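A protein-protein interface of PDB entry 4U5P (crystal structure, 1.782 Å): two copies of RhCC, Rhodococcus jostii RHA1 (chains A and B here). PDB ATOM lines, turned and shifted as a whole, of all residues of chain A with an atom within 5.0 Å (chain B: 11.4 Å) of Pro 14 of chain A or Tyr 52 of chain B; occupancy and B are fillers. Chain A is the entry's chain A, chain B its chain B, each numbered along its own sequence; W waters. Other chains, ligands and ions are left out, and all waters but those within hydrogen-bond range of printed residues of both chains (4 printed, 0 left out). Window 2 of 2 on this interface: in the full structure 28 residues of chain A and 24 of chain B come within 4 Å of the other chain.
The side-chain amino group (NZ) of Lys 17 of chain A lies within hydrogen-bond range of the backbone carbonyl oxygen (O) of Glu 49 of chain B (2.9 Å).
The backbone NH (N) of Gly 54 of chain B is in hydrogen-bond range of the backbone carbonyl oxygen (O) of Val 39 of chain A, at 2.8 Å.
The backbone NH of Val 41 of chain A lies within hydrogen-bond range of the backbone carbonyl oxygen of Tyr 52 of chain B, 2.8 Å away.
The backbone NH (N) of Phe 43 of chain A is in hydrogen-bond range of the backbone carbonyl oxygen (O) of Thr 50 of chain B.
The side-chain amide nitrogen of Asn 59 of chain B lies within hydrogen-bond range of the side-chain carboxylate of Glu 49 of chain B, 3.0 Å away.
O of Glu 18 of chain A sits at hydrogen-bond distance from OG of Ser 21 of chain A (3.1 Å).
O of Lys 17 of chain A lies within hydrogen-bond range of OG of Ser 21 of chain A, 3.1 Å away.
The side-chain hydroxyl of Thr 50 of chain B is in hydrogen-bond range of the backbone carbonyl oxygen of Pro 47 of chain B (2.7 Å).
O of Met 51 of chain B lies within hydrogen-bond range of N of Asn 58 of chain B, 2.9 Å away.
OH of Tyr 52 of chain B is in hydrogen-bond range of O of Glu 49 of chain B (3.3 Å).
Tyr 52 of chain B touches Pro 14 of chain A.
Tyr 52 of chain B touches Glu 18 of chain A (CE2 to CA, 3.9 Å).
CD2 of Tyr 52 of chain B touches OG of Ser 21 of chain A, at 3.4 Å.
OG of Ser 21 of chain A touches CA of Gly 55 of chain B, 3.4 Å away.
O of Val 39 of chain A touches O of Tyr 52 of chain B, 3.6 Å away.
Tyr 52 of chain B touches Val 40 of chain A (O to CA, 3.3 Å).
CG2 of Val 40 of chain A touches OE1 of Glu 102 of chain B (3.5 Å).
Val 41 of chain A touches Thr 50 of chain B (O to O, 3.6 Å).
Phe 43 of chain A touches Met 46 of chain B (O to CE, 3.6 Å).
Tyr 52 of chain B touches Phe 43 of chain A (CD1 to CE2, 3.7 Å).
Pro 14 of chain A touches just one residue of chain B: Tyr 52.
Of chain A, only Pro 14, Lys 17, Glu 18, Ser 21, Val 39, Val 40, Val 41 and Phe 43 come within 4 Å of Tyr 52 of chain B.
No residue of chain B comes within 4 Å of Asp 16 of chain A.
Of chain B, only Glu 49 and Tyr 52 come within 4 Å of Lys 17 of chain A.
Glu 18 of chain A touches just these residues of chain B: Tyr 52 and Gly 55.
Of chain B, only Tyr 52 (3.4 Å) and Gly 55 (3.4 Å) come within 4 Å of Ser 21 of chain A.
Of chain B, only Thr 50, Met 51 and Tyr 52 come within 4 Å of Val 41 of chain A.
Printed residues of chain A within 4 Å of Glu 49 of chain B: Lys 17.
Of the printed residues of chain A, Met 51 of chain B touches Val 41 (3.7 Å).
Printed residues of chain A within 4 Å of Phe 61 of chain B: Val 40 (3.9 Å).
Printed residues of chain A within 4 Å of Gly 54 of chain B: Val 39.
Printed residues of chain B within 4 Å of Phe 43 of chain A: Met 46, Thr 50 and Tyr 52.
Asn 60 of chain B touches none of the printed residues of chain A.
Arg 63 of chain B touches none of the printed residues of chain A.
The nearest printed residue of chain A that does not touch Tyr 52 of chain B is Thr 13 of chain A (5.4 Å).
Along chain B the printed residues that touch a printed residue of chain A span positions 46 to 102.
No position is printed for both chains.
Water W2 bridges the backbone carbonyl oxygen of Lys 48 of chain B (2.5 Å) and the side-chain amino group of Lys 17 of chain A (3.3 Å).
Water W3 lies within hydrogen-bond range of the side-chain hydroxyl (OH) of Tyr 52 of chain B, the side-chain carboxylate (OE1) of Glu 49 of chain B and the backbone carbonyl oxygen (O) of Pro 14 of chain A.
Water W1 lies within hydrogen-bond range of N of Gly 55 of chain B (2.9 Å), O of Val 39 of chain A (3.1 Å), O of Tyr 52 of chain B (3.2 Å) and N of Gly 54 of chain B (3.3 Å).
Water W4 bridges N of Ala 57 of chain B (3.0 Å) and OE1 of Glu 18 of chain A (3.0 Å).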
ATOM      1  N   PHE A  12      13.760  20.674  31.730  1.00  0.00           N
ATOM      2  CA  PHE A  12      14.345  20.538  30.397  1.00  0.00           C
ATOM      3  C   PHE A  12      13.303  20.345  29.308  1.00  0.00           C
ATOM      4  O   PHE A  12      12.398  19.522  29.439  1.00  0.00           O
ATOM      5  CB  PHE A  12      15.311  19.351  30.342  1.00  0.00           C
ATOM      6  CG  PHE A  12      16.517  19.493  31.222  1.00  0.00           C
ATOM      7  CD1 PHE A  12      17.159  20.715  31.361  1.00  0.00           C
ATOM      8  CD2 PHE A  12      17.024  18.393  31.895  1.00  0.00           C
ATOM      9  CE1 PHE A  12      18.276  20.841  32.167  1.00  0.00           C
ATOM     10  CE2 PHE A  12      18.146  18.512  32.701  1.00  0.00           C
ATOM     11  CZ  PHE A  12      18.771  19.738  32.834  1.00  0.00           C
ATOM     12  N   THR A  13      13.486  21.076  28.215  1.00  0.00           N
ATOM     13  CA  THR A  13      12.704  20.878  26.999  1.00  0.00           C
ATOM     14  C   THR A  13      13.209  19.649  26.248  1.00  0.00           C
ATOM     15  O   THR A  13      14.294  19.148  26.540  1.00  0.00           O
ATOM     16  CB  THR A  13      12.799  22.102  26.063  1.00  0.00           C
ATOM     17  OG1 THR A  13      14.166  22.307  25.683  1.00  0.00           O
ATOM     18  CG2 THR A  13      12.285  23.350  26.754  1.00  0.00           C
ATOM     19  N   PRO A  14      12.426  19.151  25.278  1.00  0.00           N
ATOM     20  CA  PRO A  14      12.930  18.056  24.448  1.00  0.00           C
ATOM     21  C   PRO A  14      14.265  18.388  23.775  1.00  0.00           C
ATOM     22  O   PRO A  14      15.128  17.510  23.702  1.00  0.00           O
ATOM     23  CB  PRO A  14      11.815  17.864  23.416  1.00  0.00           C
ATOM     24  CG  PRO A  14      10.585  18.282  24.132  1.00  0.00           C
ATOM     25  CD  PRO A  14      11.006  19.436  25.006  1.00  0.00           C
ATOM     26  N   ASP A  15      14.451  19.636  23.337  1.00  0.00           N
ATOM     27  CA  ASP A  15      15.703  20.043  22.707  1.00  0.00           C
ATOM     28  C   ASP A  15      16.857  20.005  23.708  1.00  0.00           C
ATOM     29  O   ASP A  15      17.957  19.563  23.373  1.00  0.00           O
ATOM     30  CB  ASP A  15      15.592  21.455  22.117  1.00  0.00           C
ATOM     31  CG  ASP A  15      14.765  21.502  20.845  1.00  0.00           C
ATOM     32  OD1 ASP A  15      14.516  20.436  20.241  1.00  0.00           O
ATOM     33  OD2 ASP A  15      14.372  22.618  20.442  1.00  0.00           O
ATOM     34  N   ASP A  16      16.592  20.450  24.932  1.00  0.00           N
ATOM     35  CA  ASP A  16      17.577  20.375  26.013  1.00  0.00           C
ATOM     36  C   ASP A  16      18.031  18.929  26.221  1.00  0.00           C
ATOM     37  O   ASP A  16      19.222  18.649  26.330  1.00  0.00           O
ATOM     38  CB  ASP A  16      17.000  20.895  27.341  1.00  0.00           C
ATOM     39  CG  ASP A  16      16.846  22.408  27.394  1.00  0.00           C
ATOM     40  OD1 ASP A  16      17.560  23.133  26.665  1.00  0.00           O
ATOM     41  OD2 ASP A  16      16.006  22.868  28.204  1.00  0.00           O
ATOM     42  N   LYS A  17      17.058  18.023  26.302  1.00  0.00           N
ATOM     43  CA  LYS A  17      17.331  16.621  26.618  1.00  0.00           C
ATOM     44  C   LYS A  17      18.101  15.975  25.481  1.00  0.00           C
ATOM     45  O   LYS A  17      18.998  15.155  25.699  1.00  0.00           O
ATOM     46  CB  LYS A  17      16.029  15.854  26.890  1.00  0.00           C
ATOM     47  CG  LYS A  17      15.253  16.323  28.111  1.00  0.00           C
ATOM     48  CD  LYS A  17      14.013  15.454  28.305  1.00  0.00           C
ATOM     49  CE  LYS A  17      12.848  16.228  28.866  1.00  0.00           C
ATOM     50  NZ  LYS A  17      11.586  15.474  28.635  1.00  0.00           N
ATOM     51  N   GLU A  18      17.763  16.358  24.254  1.00  0.00           N
ATOM     52  CA  GLU A  18      18.467  15.856  23.096  1.00  0.00           C
ATOM     53  C   GLU A  18      19.934  16.291  23.141  1.00  0.00           C
ATOM     54  O   GLU A  18      20.839  15.472  22.968  1.00  0.00           O
ATOM     55  CB  GLU A  18      17.807  16.361  21.806  1.00  0.00           C
ATOM     56  CG  GLU A  18      18.514  15.907  20.546  1.00  0.00           C
ATOM     57  CD  GLU A  18      17.791  16.340  19.284  1.00  0.00           C
ATOM     58  OE1 GLU A  18      16.646  15.894  19.061  1.00  0.00           O
ATOM     59  OE2 GLU A  18      18.365  17.150  18.529  1.00  0.00           O
ATOM     60  N   SER A  21      21.840  14.538  26.156  1.00  0.00           N
ATOM     61  CA  SER A  21      22.109  13.123  25.913  1.00  0.00           C
ATOM     62  C   SER A  21      23.148  12.946  24.792  1.00  0.00           C
ATOM     63  O   SER A  21      23.935  12.000  24.817  1.00  0.00           O
ATOM     64  CB  SER A  21      20.816  12.370  25.594  1.00  0.00           C
ATOM     65  OG  SER A  21      20.288  12.727  24.336  1.00  0.00           O
ATOM     66  N   VAL A  39      24.655   3.779  24.800  1.00  0.00           N
ATOM     67  CA  VAL A  39      24.449   4.856  25.773  1.00  0.00           C
ATOM     68  C   VAL A  39      22.972   5.211  25.919  1.00  0.00           C
ATOM     69  O   VAL A  39      22.361   5.768  25.009  1.00  0.00           O
ATOM     70  CB  VAL A  39      25.234   6.117  25.385  1.00  0.00           C
ATOM     71  CG1 VAL A  39      25.133   7.159  26.495  1.00  0.00           C
ATOM     72  CG2 VAL A  39      26.698   5.769  25.124  1.00  0.00           C
ATOM     73  N   VAL A  40      22.419   4.890  27.088  1.00  0.00           N
ATOM     74  CA  VAL A  40      21.026   5.145  27.408  1.00  0.00           C
ATOM     75  C   VAL A  40      20.905   6.188  28.519  1.00  0.00           C
ATOM     76  O   VAL A  40      21.542   6.059  29.562  1.00  0.00           O
ATOM     77  CB  VAL A  40      20.318   3.857  27.854  1.00  0.00           C
ATOM     78  CG1 VAL A  40      18.867   4.147  28.243  1.00  0.00           C
ATOM     79  CG2 VAL A  40      20.380   2.815  26.745  1.00  0.00           C
ATOM     80  N   VAL A  41      20.089   7.214  28.278  1.00  0.00           N
ATOM     81  CA  VAL A  41      19.842   8.270  29.257  1.00  0.00           C
ATOM     82  C   VAL A  41      18.342   8.393  29.488  1.00  0.00           C
ATOM     83  O   VAL A  41      17.566   8.603  28.551  1.00  0.00           O
ATOM     84  CB  VAL A  41      20.411   9.641  28.821  1.00  0.00           C
ATOM     85  CG1 VAL A  41      20.206  10.681  29.928  1.00  0.00           C
ATOM     86  CG2 VAL A  41      21.880   9.526  28.467  1.00  0.00           C
ATOM     87  N   PHE A  43      15.467  10.447  31.539  1.00  0.00           N
ATOM     88  CA  PHE A  43      15.099  11.670  32.244  1.00  0.00           C
ATOM     89  C   PHE A  43      13.830  11.465  33.063  1.00  0.00           C
ATOM     90  O   PHE A  43      12.802  11.034  32.534  1.00  0.00           O
ATOM     91  CB  PHE A  43      14.895  12.808  31.248  1.00  0.00           C
ATOM     92  CG  PHE A  43      16.159  13.249  30.580  1.00  0.00           C
ATOM     93  CD1 PHE A  43      16.934  14.232  31.155  1.00  0.00           C
ATOM     94  CD2 PHE A  43      16.580  12.676  29.386  1.00  0.00           C
ATOM     95  CE1 PHE A  43      18.104  14.641  30.561  1.00  0.00           C
ATOM     96  CE2 PHE A  43      17.753  13.083  28.784  1.00  0.00           C
ATOM     97  CZ  PHE A  43      18.514  14.069  29.369  1.00  0.00           C
ATOM     98  N   PHE B   6      11.310  -0.232  32.561  1.00  0.00           N
ATOM     99  CA  PHE B   6      10.947   1.067  32.021  1.00  0.00           C
ATOM    100  C   PHE B   6      10.363   0.891  30.629  1.00  0.00           C
ATOM    101  O   PHE B   6      11.049   0.384  29.753  1.00  0.00           O
ATOM    102  CB  PHE B   6      12.177   1.976  31.966  1.00  0.00           C
ATOM    103  CG  PHE B   6      12.810   2.224  33.311  1.00  0.00           C
ATOM    104  CD1 PHE B   6      13.785   1.373  33.809  1.00  0.00           C
ATOM    105  CD2 PHE B   6      12.441   3.319  34.065  1.00  0.00           C
ATOM    106  CE1 PHE B   6      14.369   1.610  35.048  1.00  0.00           C
ATOM    107  CE2 PHE B   6      13.026   3.559  35.301  1.00  0.00           C
ATOM    108  CZ  PHE B   6      13.994   2.705  35.783  1.00  0.00           C
ATOM    109  N   THR B   7       9.123   1.338  30.429  1.00  0.00           N
ATOM    110  CA  THR B   7       8.419   1.125  29.169  1.00  0.00           C
ATOM    111  C   THR B   7       7.844   2.433  28.641  1.00  0.00           C
ATOM    112  O   THR B   7       7.642   3.380  29.402  1.00  0.00           O
ATOM    113  CB  THR B   7       7.248   0.130  29.330  1.00  0.00           C
ATOM    114  OG1 THR B   7       6.173   0.768  30.028  1.00  0.00           O
ATOM    115  CG2 THR B   7       7.673  -1.117  30.102  1.00  0.00           C
ATOM    116  N   PRO B   8       7.545   2.476  27.334  1.00  0.00           N
ATOM    117  CA  PRO B   8       6.741   3.583  26.808  1.00  0.00           C
ATOM    118  C   PRO B   8       5.403   3.666  27.547  1.00  0.00           C
ATOM    119  O   PRO B   8       4.923   2.635  28.019  1.00  0.00           O
ATOM    120  CB  PRO B   8       6.546   3.208  25.328  1.00  0.00           C
ATOM    121  CG  PRO B   8       7.661   2.302  25.005  1.00  0.00           C
ATOM    122  CD  PRO B   8       7.948   1.532  26.282  1.00  0.00           C
ATOM    123  N   MET B  46       7.293   5.639  30.936  1.00  0.00           N
ATOM    124  CA  MET B  46       8.126   6.766  30.556  1.00  0.00           C
ATOM    125  C   MET B  46       7.482   7.505  29.389  1.00  0.00           C
ATOM    126  O   MET B  46       7.316   6.921  28.316  1.00  0.00           O
ATOM    127  CB  MET B  46       9.519   6.285  30.167  1.00  0.00           C
ATOM    128  CG  MET B  46      10.266   5.612  31.294  1.00  0.00           C
ATOM    129  SD  MET B  46      10.773   6.773  32.580  1.00  0.00           S
ATOM    130  CE  MET B  46      12.127   7.614  31.750  1.00  0.00           C
ATOM    131  N   PRO B  47       7.096   8.778  29.588  1.00  0.00           N
ATOM    132  CA  PRO B  47       6.477   9.521  28.475  1.00  0.00           C
ATOM    133  C   PRO B  47       7.399   9.702  27.287  1.00  0.00           C
ATOM    134  O   PRO B  47       8.605   9.502  27.405  1.00  0.00           O
ATOM    135  CB  PRO B  47       6.161  10.889  29.092  1.00  0.00           C
ATOM    136  CG  PRO B  47       6.150  10.667  30.554  1.00  0.00           C
ATOM    137  CD  PRO B  47       7.148   9.584  30.815  1.00  0.00           C
ATOM    138  N   LYS B  48       6.838  10.098  26.146  1.00  0.00           N
ATOM    139  CA  LYS B  48       7.660  10.377  24.980  1.00  0.00           C
ATOM    140  C   LYS B  48       8.699  11.442  25.302  1.00  0.00           C
ATOM    141  O   LYS B  48       8.460  12.347  26.102  1.00  0.00           O
ATOM    142  CB  LYS B  48       6.814  10.824  23.781  1.00  0.00           C
ATOM    143  CG  LYS B  48       5.953   9.724  23.185  1.00  0.00           C
ATOM    144  CD  LYS B  48       5.175  10.225  21.985  1.00  0.00           C
ATOM    145  CE  LYS B  48       4.281   9.135  21.419  1.00  0.00           C
ATOM    146  NZ  LYS B  48       3.387   9.650  20.346  1.00  0.00           N
ATOM    147  N   GLU B  49       9.848  11.314  24.652  1.00  0.00           N
ATOM    148  CA  GLU B  49      10.971  12.239  24.807  1.00  0.00           C
ATOM    149  C   GLU B  49      11.569  12.217  26.224  1.00  0.00           C
ATOM    150  O   GLU B  49      11.983  13.257  26.740  1.00  0.00           O
ATOM    151  CB  GLU B  49      10.545  13.671  24.447  1.00  0.00           C
ATOM    152  CG  GLU B  49       9.623  13.771  23.236  1.00  0.00           C
ATOM    153  CD  GLU B  49      10.176  13.064  22.021  1.00  0.00           C
ATOM    154  OE1 GLU B  49      11.397  13.165  21.765  1.00  0.00           O
ATOM    155  OE2 GLU B  49       9.384  12.393  21.327  1.00  0.00           O
ATOM    156  N   THR B  50      11.631  11.038  26.839  1.00  0.00           N
ATOM    157  CA  THR B  50      12.305  10.907  28.139  1.00  0.00           C
ATOM    158  C   THR B  50      13.365   9.807  28.123  1.00  0.00           C
ATOM    159  O   THR B  50      14.225   9.783  29.000  1.00  0.00           O
ATOM    160  CB  THR B  50      11.303  10.623  29.307  1.00  0.00           C
ATOM    161  OG1 THR B  50      10.683   9.340  29.156  1.00  0.00           O
ATOM    162  CG2 THR B  50      10.241  11.709  29.398  1.00  0.00           C
ATOM    163  N   MET B  51      13.311   8.906  27.140  1.00  0.00           N
ATOM    164  CA  MET B  51      14.310   7.833  26.999  1.00  0.00           C
ATOM    165  C   MET B  51      15.160   8.069  25.748  1.00  0.00           C
ATOM    166  O   MET B  51      14.647   8.003  24.631  1.00  0.00           O
ATOM    167  CB  MET B  51      13.642   6.451  26.902  1.00  0.00           C
ATOM    168  CG  MET B  51      12.682   6.104  28.050  1.00  0.00           C
ATOM    169  SD  MET B  51      11.902   4.461  27.972  1.00  0.00           S
ATOM    170  CE  MET B  51      13.297   3.401  28.328  1.00  0.00           C
ATOM    171  N   TYR B  52      16.459   8.311  25.943  1.00  0.00           N
ATOM    172  CA  TYR B  52      17.372   8.650  24.850  1.00  0.00           C
ATOM    173  C   TYR B  52      18.416   7.562  24.661  1.00  0.00           C
ATOM    174  O   TYR B  52      19.111   7.183  25.603  1.00  0.00           O
ATOM    175  CB  TYR B  52      18.036  10.007  25.123  1.00  0.00           C
ATOM    176  CG  TYR B  52      17.040  11.130  24.973  1.00  0.00           C
ATOM    177  CD1 TYR B  52      16.110  11.403  25.973  1.00  0.00           C
ATOM    178  CD2 TYR B  52      16.989  11.879  23.807  1.00  0.00           C
ATOM    179  CE1 TYR B  52      15.176  12.412  25.820  1.00  0.00           C
ATOM    180  CE2 TYR B  52      16.062  12.886  23.643  1.00  0.00           C
ATOM    181  CZ  TYR B  52      15.156  13.148  24.646  1.00  0.00           C
ATOM    182  OH  TYR B  52      14.239  14.159  24.467  1.00  0.00           O
ATOM    183  N   VAL B  53      18.495   7.043  23.440  1.00  0.00           N
ATOM    184  CA  VAL B  53      19.448   5.999  23.096  1.00  0.00           C
ATOM    185  C   VAL B  53      20.414   6.560  22.066  1.00  0.00           C
ATOM    186  O   VAL B  53      19.995   6.983  20.994  1.00  0.00           O
ATOM    187  CB  VAL B  53      18.744   4.743  22.543  1.00  0.00           C
ATOM    188  CG1 VAL B  53      19.770   3.698  22.113  1.00  0.00           C
ATOM    189  CG2 VAL B  53      17.753   4.169  23.584  1.00  0.00           C
ATOM    190  N   GLY B  54      21.698   6.592  22.403  1.00  0.00           N
ATOM    191  CA  GLY B  54      22.698   7.138  21.502  1.00  0.00           C
ATOM    192  C   GLY B  54      22.439   8.580  21.118  1.00  0.00           C
ATOM    193  O   GLY B  54      22.786   9.007  20.007  1.00  0.00           O
ATOM    194  N   GLY B  55      21.811   9.322  22.025  1.00  0.00           N
ATOM    195  CA  GLY B  55      21.607  10.755  21.863  1.00  0.00           C
ATOM    196  C   GLY B  55      20.325  11.147  21.153  1.00  0.00           C
ATOM    197  O   GLY B  55      20.122  12.320  20.828  1.00  0.00           O
ATOM    198  N   LYS B  56      19.465  10.164  20.902  1.00  0.00           N
ATOM    199  CA  LYS B  56      18.208  10.380  20.208  1.00  0.00           C
ATOM    200  C   LYS B  56      17.077   9.735  20.996  1.00  0.00           C
ATOM    201  O   LYS B  56      17.207   8.609  21.454  1.00  0.00           O
ATOM    202  CB  LYS B  56      18.267   9.758  18.806  1.00  0.00           C
ATOM    203  CG  LYS B  56      19.322  10.326  17.885  1.00  0.00           C
ATOM    204  CD  LYS B  56      19.027   9.941  16.437  1.00  0.00           C
ATOM    205  CE  LYS B  56      19.898  10.703  15.447  1.00  0.00           C
ATOM    206  NZ  LYS B  56      21.277  10.120  15.391  1.00  0.00           N
ATOM    207  N   ALA B  57      15.949  10.420  21.116  1.00  0.00           N
ATOM    208  CA  ALA B  57      14.792   9.830  21.778  1.00  0.00           C
ATOM    209  C   ALA B  57      14.390   8.546  21.069  1.00  0.00           C
ATOM    210  O   ALA B  57      14.281   8.504  19.837  1.00  0.00           O
ATOM    211  CB  ALA B  57      13.634  10.801  21.795  1.00  0.00           C
ATOM    212  N   ASN B  58      14.199   7.497  21.860  1.00  0.00           N
ATOM    213  CA  ASN B  58      13.610   6.253  21.390  1.00  0.00           C
ATOM    214  C   ASN B  58      12.344   5.985  22.192  1.00  0.00           C
ATOM    215  O   ASN B  58      12.389   5.627  23.374  1.00  0.00           O
ATOM    216  CB  ASN B  58      14.589   5.090  21.499  1.00  0.00           C
ATOM    217  CG  ASN B  58      14.078   3.826  20.815  1.00  0.00           C
ATOM    218  OD1 ASN B  58      12.880   3.656  20.621  1.00  0.00           O
ATOM    219  ND2 ASN B  58      14.989   2.919  20.475  1.00  0.00           N
ATOM    220  N   ASN B  59      11.205   6.211  21.549  1.00  0.00           N
ATOM    221  CA  ASN B  59       9.909   6.068  22.200  1.00  0.00           C
ATOM    222  C   ASN B  59       9.362   4.654  22.055  1.00  0.00           C
ATOM    223  O   ASN B  59       8.202   4.393  22.384  1.00  0.00           O
ATOM    224  CB  ASN B  59       8.925   7.088  21.621  1.00  0.00           C
ATOM    225  CG  ASN B  59       9.376   8.524  21.838  1.00  0.00           C
ATOM    226  OD1 ASN B  59      10.024   8.843  22.840  1.00  0.00           O
ATOM    227  ND2 ASN B  59       9.049   9.395  20.887  1.00  0.00           N
ATOM    228  N   ASN B  60      10.207   3.753  21.562  1.00  0.00           N
ATOM    229  CA  ASN B  60       9.834   2.362  21.316  1.00  0.00           C
ATOM    230  C   ASN B  60      10.797   1.420  22.027  1.00  0.00           C
ATOM    231  O   ASN B  60      11.144   0.360  21.509  1.00  0.00           O
ATOM    232  CB  ASN B  60       9.837   2.077  19.804  1.00  0.00           C
ATOM    233  CG  ASN B  60       9.284   0.702  19.463  1.00  0.00           C
ATOM    234  OD1 ASN B  60       8.282   0.266  20.030  1.00  0.00           O
ATOM    235  ND2 ASN B  60       9.959   0.000  18.563  1.00  0.00           N
ATOM    236  N   PHE B  61      11.208   1.802  23.231  1.00  0.00           N
ATOM    237  CA  PHE B  61      12.347   1.168  23.904  1.00  0.00           C
ATOM    238  C   PHE B  61      11.970   0.737  25.322  1.00  0.00           C
ATOM    239  O   PHE B  61      11.406   1.517  26.087  1.00  0.00           O
ATOM    240  CB  PHE B  61      13.525   2.138  23.936  1.00  0.00           C
ATOM    241  CG  PHE B  61      14.793   1.573  24.534  1.00  0.00           C
ATOM    242  CD1 PHE B  61      15.355   0.406  24.051  1.00  0.00           C
ATOM    243  CD2 PHE B  61      15.441   2.243  25.555  1.00  0.00           C
ATOM    244  CE1 PHE B  61      16.540  -0.099  24.592  1.00  0.00           C
ATOM    245  CE2 PHE B  61      16.621   1.749  26.097  1.00  0.00           C
ATOM    246  CZ  PHE B  61      17.169   0.573  25.608  1.00  0.00           C
ATOM    247  N   VAL B  62      12.241  -0.525  25.644  1.00  0.00           N
ATOM    248  CA  VAL B  62      12.037  -1.054  26.993  1.00  0.00           C
ATOM    249  C   VAL B  62      13.396  -1.343  27.621  1.00  0.00           C
ATOM    250  O   VAL B  62      14.170  -2.124  27.080  1.00  0.00           O
ATOM    251  CB  VAL B  62      11.174  -2.331  26.981  1.00  0.00           C
ATOM    252  CG1 VAL B  62      11.079  -2.937  28.380  1.00  0.00           C
ATOM    253  CG2 VAL B  62       9.778  -2.021  26.434  1.00  0.00           C
ATOM    254  N   ARG B  63      13.689  -0.703  28.752  1.00  0.00           N
ATOM    255  CA  ARG B  63      14.963  -0.893  29.427  1.00  0.00           C
ATOM    256  C   ARG B  63      14.714  -1.626  30.741  1.00  0.00           C
ATOM    257  O   ARG B  63      13.865  -1.212  31.538  1.00  0.00           O
ATOM    258  CB  ARG B  63      15.657   0.446  29.663  1.00  0.00           C
ATOM    259  CG  ARG B  63      17.094   0.344  30.171  1.00  0.00           C
ATOM    260  CD  ARG B  63      17.960  -0.440  29.199  1.00  0.00           C
ATOM    261  NE  ARG B  63      19.395  -0.357  29.458  1.00  0.00           N
ATOM    262  CZ  ARG B  63      20.050  -1.084  30.356  1.00  0.00           C
ATOM    263  NH1 ARG B  63      19.391  -1.936  31.134  1.00  0.00           N
ATOM    264  NH2 ARG B  63      21.369  -0.934  30.488  1.00  0.00           N
ATOM    265  N   ASP B 100      12.392  -2.309  20.965  1.00  0.00           N
ATOM    266  CA  ASP B 100      13.829  -2.433  21.188  1.00  0.00           C
ATOM    267  C   ASP B 100      14.001  -2.663  22.682  1.00  0.00           C
ATOM    268  O   ASP B 100      13.187  -2.184  23.459  1.00  0.00           O
ATOM    269  CB  ASP B 100      14.570  -1.189  20.735  1.00  0.00           C
ATOM    270  CG  ASP B 100      14.436  -0.952  19.243  1.00  0.00           C
ATOM    271  OD1 ASP B 100      14.405  -1.952  18.486  1.00  0.00           O
ATOM    272  OD2 ASP B 100      14.341   0.232  18.850  1.00  0.00           O
ATOM    273  N   GLU B 102      16.945  -3.791  26.195  1.00  0.00           N
ATOM    274  CA  GLU B 102      18.264  -4.045  26.765  1.00  0.00           C
ATOM    275  C   GLU B 102      18.069  -4.401  28.223  1.00  0.00           C
ATOM    276  O   GLU B 102      17.139  -3.902  28.838  1.00  0.00           O
ATOM    277  CB  GLU B 102      19.165  -2.822  26.626  1.00  0.00           C
ATOM    278  CG  GLU B 102      20.561  -2.985  27.189  1.00  0.00           C
ATOM    279  CD  GLU B 102      21.453  -1.795  26.867  1.00  0.00           C
ATOM    280  OE1 GLU B 102      20.953  -0.645  26.810  1.00  0.00           O
ATOM    281  OE2 GLU B 102      22.658  -2.020  26.654  1.00  0.00           O
HETATM  282  O   HOH W   1      21.749   8.820  24.885  1.00  0.00           O
HETATM  283  O   HOH W   2       8.675  14.371  27.531  1.00  0.00           O
HETATM  284  O   HOH W   3      13.973  15.039  21.722  1.00  0.00           O
HETATM  285  O   HOH W   4      15.632  13.198  20.033  1.00  0.00           O
